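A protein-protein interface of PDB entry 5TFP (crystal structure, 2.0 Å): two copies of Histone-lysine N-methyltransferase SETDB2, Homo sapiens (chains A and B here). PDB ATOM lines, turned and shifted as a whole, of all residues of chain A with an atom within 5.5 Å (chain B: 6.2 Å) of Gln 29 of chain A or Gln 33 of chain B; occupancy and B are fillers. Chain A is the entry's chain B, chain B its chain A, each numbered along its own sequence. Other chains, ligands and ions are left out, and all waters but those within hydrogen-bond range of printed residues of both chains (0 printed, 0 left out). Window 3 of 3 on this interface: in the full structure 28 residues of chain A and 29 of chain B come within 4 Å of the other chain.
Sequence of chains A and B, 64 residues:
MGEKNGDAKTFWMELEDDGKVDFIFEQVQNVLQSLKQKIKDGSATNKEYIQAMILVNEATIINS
NE2 of Gln 29 of chain B sits close to NE2 of Gln 29 of chain A, at 2.9 Å.
NE2 of Gln 29 of chain A lies close to NE2 of Gln 33 of chain B, 2.9 Å away.
The side-chain amide oxygen (OE1) of Gln 29 of chain A lies close to the backbone carbonyl oxygen (O) of Phe 25 of chain A.
Among the printed residues, pairs that only touch across the chains: Phe 25 of chain A with Leu 32 of chain B, Phe 25 of chain A with Lys 36 of chain B, Val 28 of chain A with Leu 32 of chain B, Leu 32 of chain A with Val 28 of chain B and Leu 32 of chain A with Leu 32 of chain B.
Of the printed residues of chain B, Val 28 of chain A touches Leu 32 (3.5 Å).
Printed residues of chain B within 4 Å of Gln 29 of chain A: Gln 29 and Gln 33.
Of the printed residues of chain A, Gln 29 of chain B touches Gln 29 (2.9 Å).
Printed residues of chain A within 4 Å of Gln 33 of chain B: Gln 29 (2.9 Å).
The nearest printed residue of chain A that does not touch Val 28 of chain B is Val 28 of chain A (6.6 Å).
Of the 11 printed residues of chain A, 4 touch a printed residue of chain B.
Hydrophobic or aromatic side chains of chain A that line the printed part of chain B: Phe 25, Val 28 and Leu 32.
Of the 11 printed residues of chain B, 5 touch a printed residue of chain A.
Hydrophobic or aromatic side chains of chain B within 4 Å of the printed part of chain A: Val 28 and Leu 32.
Among the printed residues, 7 pairs touch across the chains.
Among the printed residues, no Asp or Glu carboxylate lies within 4 Å of a Lys or Arg side-chain nitrogen of the other chain.
Val 28 of chain A touches Leu 32 of chain B, and with the chains exchanged Leu 32 of chain A touches Val 28 of chain B.
Gln 29 of chain A touches its own counterpart, Gln 29 of chain B.
Gln 29 of chain A touches Gln 33 of chain B, but with the chains exchanged Gln 33 of chain A does not touch Gln 29 of chain B (7.0 Å).
Leu 32 of chain B touches its own counterpart, Leu 32 of chain A.
Positions printed for both chains: 28, 29, 30, 31, 32, 33 and 34.
Of the 7 pairs that touch across the chains among the printed residues, 4 have their exchanged pair printed and touching as well.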
ATOM      1  N   ILE A  24     -26.892   5.732 -18.559  1.00  0.00           N
ATOM      2  CA  ILE A  24     -25.962   4.604 -18.581  1.00  0.00           C
ATOM      3  C   ILE A  24     -25.162   4.539 -17.266  1.00  0.00           C
ATOM      4  O   ILE A  24     -24.949   3.453 -16.714  1.00  0.00           O
ATOM      5  CB  ILE A  24     -24.995   4.658 -19.819  1.00  0.00           C
ATOM      6  CG1 ILE A  24     -24.285   3.311 -19.996  1.00  0.00           C
ATOM      7  CG2 ILE A  24     -23.988   5.809 -19.740  1.00  0.00           C
ATOM      8  CD1 ILE A  24     -25.166   2.278 -20.722  1.00  0.00           C
ATOM      9  N   PHE A  25     -24.761   5.688 -16.732  1.00  0.00           N
ATOM     10  CA  PHE A  25     -24.069   5.679 -15.444  1.00  0.00           C
ATOM     11  C   PHE A  25     -24.986   5.188 -14.309  1.00  0.00           C
ATOM     12  O   PHE A  25     -24.526   4.487 -13.409  1.00  0.00           O
ATOM     13  CB  PHE A  25     -23.468   7.064 -15.138  1.00  0.00           C
ATOM     14  CG  PHE A  25     -22.099   7.237 -15.732  1.00  0.00           C
ATOM     15  CD1 PHE A  25     -20.975   6.755 -15.060  1.00  0.00           C
ATOM     16  CD2 PHE A  25     -21.938   7.798 -17.002  1.00  0.00           C
ATOM     17  CE1 PHE A  25     -19.701   6.878 -15.619  1.00  0.00           C
ATOM     18  CE2 PHE A  25     -20.675   7.926 -17.582  1.00  0.00           C
ATOM     19  CZ  PHE A  25     -19.548   7.461 -16.897  1.00  0.00           C
ATOM     20  N   GLU A  26     -26.267   5.534 -14.363  1.00  0.00           N
ATOM     21  CA  GLU A  26     -27.223   5.026 -13.376  1.00  0.00           C
ATOM     22  C   GLU A  26     -27.326   3.497 -13.430  1.00  0.00           C
ATOM     23  O   GLU A  26     -27.422   2.835 -12.389  1.00  0.00           O
ATOM     24  CB  GLU A  26     -28.607   5.656 -13.579  1.00  0.00           C
ATOM     25  CG  GLU A  26     -28.712   7.106 -13.142  1.00  0.00           C
ATOM     26  CD  GLU A  26     -29.943   7.818 -13.724  1.00  0.00           C
ATOM     27  OE1 GLU A  26     -30.887   7.123 -14.156  1.00  0.00           O
ATOM     28  OE2 GLU A  26     -29.962   9.073 -13.760  1.00  0.00           O
ATOM     29  N   GLN A  27     -27.296   2.935 -14.638  1.00  0.00           N
ATOM     30  CA  GLN A  27     -27.341   1.481 -14.804  1.00  0.00           C
ATOM     31  C   GLN A  27     -26.097   0.827 -14.206  1.00  0.00           C
ATOM     32  O   GLN A  27     -26.175  -0.223 -13.565  1.00  0.00           O
ATOM     33  CB  GLN A  27     -27.466   1.103 -16.280  1.00  0.00           C
ATOM     34  CG  GLN A  27     -28.683   1.700 -16.950  1.00  0.00           C
ATOM     35  CD  GLN A  27     -29.962   1.416 -16.177  1.00  0.00           C
ATOM     36  OE1 GLN A  27     -30.333   0.261 -15.979  1.00  0.00           O
ATOM     37  NE2 GLN A  27     -30.629   2.470 -15.721  1.00  0.00           N
ATOM     38  N   VAL A  28     -24.951   1.457 -14.414  1.00  0.00           N
ATOM     39  CA  VAL A  28     -23.703   0.935 -13.874  1.00  0.00           C
ATOM     40  C   VAL A  28     -23.777   0.987 -12.344  1.00  0.00           C
ATOM     41  O   VAL A  28     -23.383   0.028 -11.659  1.00  0.00           O
ATOM     42  CB  VAL A  28     -22.473   1.708 -14.398  1.00  0.00           C
ATOM     43  CG1 VAL A  28     -21.195   1.285 -13.632  1.00  0.00           C
ATOM     44  CG2 VAL A  28     -22.308   1.500 -15.941  1.00  0.00           C
ATOM     45  N   GLN A  29     -24.302   2.092 -11.822  1.00  0.00           N
ATOM     46  CA  GLN A  29     -24.414   2.277 -10.385  1.00  0.00           C
ATOM     47  C   GLN A  29     -25.382   1.271  -9.762  1.00  0.00           C
ATOM     48  O   GLN A  29     -25.152   0.790  -8.651  1.00  0.00           O
ATOM     49  CB  GLN A  29     -24.843   3.722 -10.075  1.00  0.00           C
ATOM     50  CG  GLN A  29     -23.752   4.766 -10.386  1.00  0.00           C
ATOM     51  CD  GLN A  29     -24.261   6.217 -10.432  1.00  0.00           C
ATOM     52  OE1 GLN A  29     -25.417   6.491 -10.775  1.00  0.00           O
ATOM     53  NE2 GLN A  29     -23.384   7.150 -10.092  1.00  0.00           N
ATOM     54  N   ASN A  30     -26.458   0.942 -10.475  1.00  0.00           N
ATOM     55  CA  ASN A  30     -27.411  -0.053 -10.004  1.00  0.00           C
ATOM     56  C   ASN A  30     -26.787  -1.464  -9.962  1.00  0.00           C
ATOM     57  O   ASN A  30     -26.988  -2.222  -8.999  1.00  0.00           O
ATOM     58  CB  ASN A  30     -28.667  -0.053 -10.879  1.00  0.00           C
ATOM     59  CG  ASN A  30     -29.531   1.173 -10.657  1.00  0.00           C
ATOM     60  OD1 ASN A  30     -29.370   1.895  -9.673  1.00  0.00           O
ATOM     61  ND2 ASN A  30     -30.467   1.405 -11.567  1.00  0.00           N
ATOM     62  N   VAL A  31     -26.007  -1.790 -10.988  1.00  0.00           N
ATOM     63  CA  VAL A  31     -25.304  -3.063 -11.037  1.00  0.00           C
ATOM     64  C   VAL A  31     -24.296  -3.147  -9.876  1.00  0.00           C
ATOM     65  O   VAL A  31     -24.224  -4.159  -9.198  1.00  0.00           O
ATOM     66  CB  VAL A  31     -24.589  -3.260 -12.413  1.00  0.00           C
ATOM     67  CG1 VAL A  31     -23.566  -4.420 -12.353  1.00  0.00           C
ATOM     68  CG2 VAL A  31     -25.620  -3.524 -13.511  1.00  0.00           C
ATOM     69  N   LEU A  32     -23.533  -2.084  -9.630  1.00  0.00           N
ATOM     70  CA  LEU A  32     -22.562  -2.110  -8.524  1.00  0.00           C
ATOM     71  C   LEU A  32     -23.230  -2.275  -7.157  1.00  0.00           C
ATOM     72  O   LEU A  32     -22.741  -3.017  -6.302  1.00  0.00           O
ATOM     73  CB  LEU A  32     -21.701  -0.829  -8.512  1.00  0.00           C
ATOM     74  CG  LEU A  32     -20.670  -0.743  -9.647  1.00  0.00           C
ATOM     75  CD1 LEU A  32     -20.204   0.670  -9.704  1.00  0.00           C
ATOM     76  CD2 LEU A  32     -19.464  -1.683  -9.415  1.00  0.00           C
ATOM     77  N   GLN A  33     -24.330  -1.561  -6.944  1.00  0.00           N
ATOM     78  CA  GLN A  33     -25.082  -1.679  -5.712  1.00  0.00           C
ATOM     79  C   GLN A  33     -25.549  -3.128  -5.514  1.00  0.00           C
ATOM     80  O   GLN A  33     -25.377  -3.710  -4.437  1.00  0.00           O
ATOM     81  CB  GLN A  33     -26.277  -0.720  -5.725  1.00  0.00           C
ATOM     82  CG  GLN A  33     -27.086  -0.709  -4.439  1.00  0.00           C
ATOM     83  CD  GLN A  33     -26.230  -0.473  -3.200  1.00  0.00           C
ATOM     84  OE1 GLN A  33     -25.386   0.425  -3.174  1.00  0.00           O
ATOM     85  NE2 GLN A  33     -26.445  -1.286  -2.166  1.00  0.00           N
ATOM     86  N   SER A  34     -26.104  -3.702  -6.575  1.00  0.00           N
ATOM     87  CA  SER A  34     -26.601  -5.074  -6.556  1.00  0.00           C
ATOM     88  C   SER A  34     -25.490  -6.059  -6.224  1.00  0.00           C
ATOM     89  O   SER A  34     -25.682  -6.965  -5.416  1.00  0.00           O
ATOM     90  CB  SER A  34     -27.224  -5.430  -7.910  1.00  0.00           C
ATOM     91  OG  SER A  34     -27.649  -6.777  -7.933  1.00  0.00           O
ATOM     92  N   VAL B  28     -14.786   2.793  -5.931  1.00  0.00           N
ATOM     93  CA  VAL B  28     -15.269   2.628  -7.308  1.00  0.00           C
ATOM     94  C   VAL B  28     -16.315   3.686  -7.682  1.00  0.00           C
ATOM     95  O   VAL B  28     -16.327   4.222  -8.801  1.00  0.00           O
ATOM     96  CB  VAL B  28     -15.880   1.206  -7.543  1.00  0.00           C
ATOM     97  CG1 VAL B  28     -16.498   1.097  -8.955  1.00  0.00           C
ATOM     98  CG2 VAL B  28     -14.778   0.127  -7.356  1.00  0.00           C
ATOM     99  N   GLN B  29     -17.209   3.966  -6.745  1.00  0.00           N
ATOM    100  CA  GLN B  29     -18.236   4.976  -6.948  1.00  0.00           C
ATOM    101  C   GLN B  29     -17.613   6.365  -7.127  1.00  0.00           C
ATOM    102  O   GLN B  29     -18.079   7.142  -7.955  1.00  0.00           O
ATOM    103  CB  GLN B  29     -19.236   4.976  -5.787  1.00  0.00           C
ATOM    104  CG  GLN B  29     -20.381   5.982  -5.948  1.00  0.00           C
ATOM    105  CD  GLN B  29     -21.207   5.765  -7.229  1.00  0.00           C
ATOM    106  OE1 GLN B  29     -21.216   4.676  -7.821  1.00  0.00           O
ATOM    107  NE2 GLN B  29     -21.908   6.809  -7.654  1.00  0.00           N
ATOM    108  N   ASN B  30     -16.566   6.678  -6.366  1.00  0.00           N
ATOM    109  CA  ASN B  30     -15.883   7.948  -6.555  1.00  0.00           C
ATOM    110  C   ASN B  30     -15.284   8.059  -7.954  1.00  0.00           C
ATOM    111  O   ASN B  30     -15.384   9.108  -8.600  1.00  0.00           O
ATOM    112  CB  ASN B  30     -14.783   8.141  -5.522  1.00  0.00           C
ATOM    113  CG  ASN B  30     -15.322   8.520  -4.180  1.00  0.00           C
ATOM    114  OD1 ASN B  30     -16.423   9.052  -4.072  1.00  0.00           O
ATOM    115  ND2 ASN B  30     -14.556   8.250  -3.144  1.00  0.00           N
ATOM    116  N   VAL B  31     -14.653   6.982  -8.415  1.00  0.00           N
ATOM    117  CA  VAL B  31     -14.076   6.970  -9.759  1.00  0.00           C
ATOM    118  C   VAL B  31     -15.166   7.153 -10.837  1.00  0.00           C
ATOM    119  O   VAL B  31     -14.996   7.931 -11.775  1.00  0.00           O
ATOM    120  CB  VAL B  31     -13.280   5.663 -10.035  1.00  0.00           C
ATOM    121  CG1 VAL B  31     -12.951   5.511 -11.548  1.00  0.00           C
ATOM    122  CG2 VAL B  31     -11.967   5.665  -9.233  1.00  0.00           C
ATOM    123  N   LEU B  32     -16.279   6.428 -10.707  1.00  0.00           N
ATOM    124  CA  LEU B  32     -17.396   6.596 -11.622  1.00  0.00           C
ATOM    125  C   LEU B  32     -17.968   7.998 -11.694  1.00  0.00           C
ATOM    126  O   LEU B  32     -18.327   8.471 -12.772  1.00  0.00           O
ATOM    127  CB  LEU B  32     -18.558   5.674 -11.234  1.00  0.00           C
ATOM    128  CG  LEU B  32     -18.621   4.268 -11.796  1.00  0.00           C
ATOM    129  CD1 LEU B  32     -19.991   3.736 -11.433  1.00  0.00           C
ATOM    130  CD2 LEU B  32     -18.404   4.272 -13.295  1.00  0.00           C
ATOM    131  N   GLN B  33     -18.168   8.609 -10.535  1.00  0.00           N
ATOM    132  CA  GLN B  33     -18.721   9.954 -10.495  1.00  0.00           C
ATOM    133  C   GLN B  33     -17.765  10.938 -11.154  1.00  0.00           C
ATOM    134  O   GLN B  33     -18.190  11.877 -11.831  1.00  0.00           O
ATOM    135  CB  GLN B  33     -18.988  10.399  -9.061  1.00  0.00           C
ATOM    136  CG  GLN B  33     -20.309   9.982  -8.505  1.00  0.00           C
ATOM    137  CD  GLN B  33     -21.478  10.621  -9.240  1.00  0.00           C
ATOM    138  OE1 GLN B  33     -21.615  11.849  -9.307  1.00  0.00           O
ATOM    139  NE2 GLN B  33     -22.331   9.783  -9.788  1.00  0.00           N
ATOM    140  N   SER B  34     -16.471  10.730 -10.935  1.00  0.00           N
ATOM    141  CA  SER B  34     -15.459  11.597 -11.529  1.00  0.00           C
ATOM    142  C   SER B  34     -15.454  11.472 -13.048  1.00  0.00           C
ATOM    143  O   SER B  34     -15.426  12.482 -13.759  1.00  0.00           O
ATOM    144  CB  SER B  34     -14.085  11.267 -10.961  1.00  0.00           C
ATOM    145  OG  SER B  34     -13.849  12.042  -9.812  1.00  0.00           O
ATOM    146  N   LEU B  35     -15.479  10.229 -13.537  1.00  0.00           N
ATOM    147  CA  LEU B  35     -15.481   9.970 -14.967  1.00  0.00           C
ATOM    148  C   LEU B  35     -16.710  10.569 -15.602  1.00  0.00           C
ATOM    149  O   LEU B  35     -16.641  11.195 -16.650  1.00  0.00           O
ATOM    150  CB  LEU B  35     -15.451   8.460 -15.263  1.00  0.00           C
ATOM    151  CG  LEU B  35     -14.131   7.741 -15.040  1.00  0.00           C
ATOM    152  CD1 LEU B  35     -14.298   6.216 -15.219  1.00  0.00           C
ATOM    153  CD2 LEU B  35     -13.110   8.259 -16.021  1.00  0.00           C
ATOM    154  N   LYS B  36     -17.849  10.360 -14.959  1.00  0.00           N
ATOM    155  CA  LYS B  36     -19.093  10.888 -15.498  1.00  0.00           C
ATOM    156  C   LYS B  36     -19.020  12.413 -15.647  1.00  0.00           C
ATOM    157  O   LYS B  36     -19.451  12.991 -16.664  1.00  0.00           O
ATOM    158  CB  LYS B  36     -20.262  10.495 -14.612  1.00  0.00           C
ATOM    159  CG  LYS B  36     -21.561  11.092 -15.103  1.00  0.00           C
ATOM    160  CD  LYS B  36     -22.781  10.498 -14.439  1.00  0.00           C
ATOM    161  CE  LYS B  36     -23.132  11.192 -13.151  1.00  0.00           C
ATOM    162  NZ  LYS B  36     -24.633  11.182 -12.915  1.00  0.00           N
ATOM    163  N   GLN B  37     -18.496  13.078 -14.628  1.00  0.00           N
ATOM    164  CA  GLN B  37     -18.444  14.519 -14.693  1.00  0.00           C
ATOM    165  C   GLN B  37     -17.445  15.002 -15.755  1.00  0.00           C
ATOM    166  O   GLN B  37     -17.697  16.011 -16.422  1.00  0.00           O
ATOM    167  CB  GLN B  37     -18.098  15.115 -13.333  1.00  0.00           C
ATOM    168  CG  GLN B  37     -18.337  16.610 -13.293  1.00  0.00           C
ATOM    169  CD  GLN B  37     -19.811  16.910 -13.477  1.00  0.00           C
ATOM    170  OE1 GLN B  37     -20.662  16.370 -12.761  1.00  0.00           O
ATOM    171  NE2 GLN B  37     -20.121  17.742 -14.454  1.00  0.00           N
ATOM    172  N   LYS B  38     -16.320  14.309 -15.918  1.00  0.00           N
ATOM    173  CA  LYS B  38     -15.339  14.749 -16.923  1.00  0.00           C
ATOM    174  C   LYS B  38     -15.857  14.522 -18.337  1.00  0.00           C
ATOM    175  O   LYS B  38     -15.535  15.281 -19.246  1.00  0.00           O
ATOM    176  CB  LYS B  38     -13.986  14.049 -16.745  1.00  0.00           C
ATOM    177  CG  LYS B  38     -13.275  14.485 -15.463  1.00  0.00           C
ATOM    178  CD  LYS B  38     -11.917  13.823 -15.320  1.00  0.00           C
ATOM    179  CE  LYS B  38     -10.850  14.671 -15.976  1.00  0.00           C
ATOM    180  NZ  LYS B  38      -9.475  14.154 -15.733  1.00  0.00           N
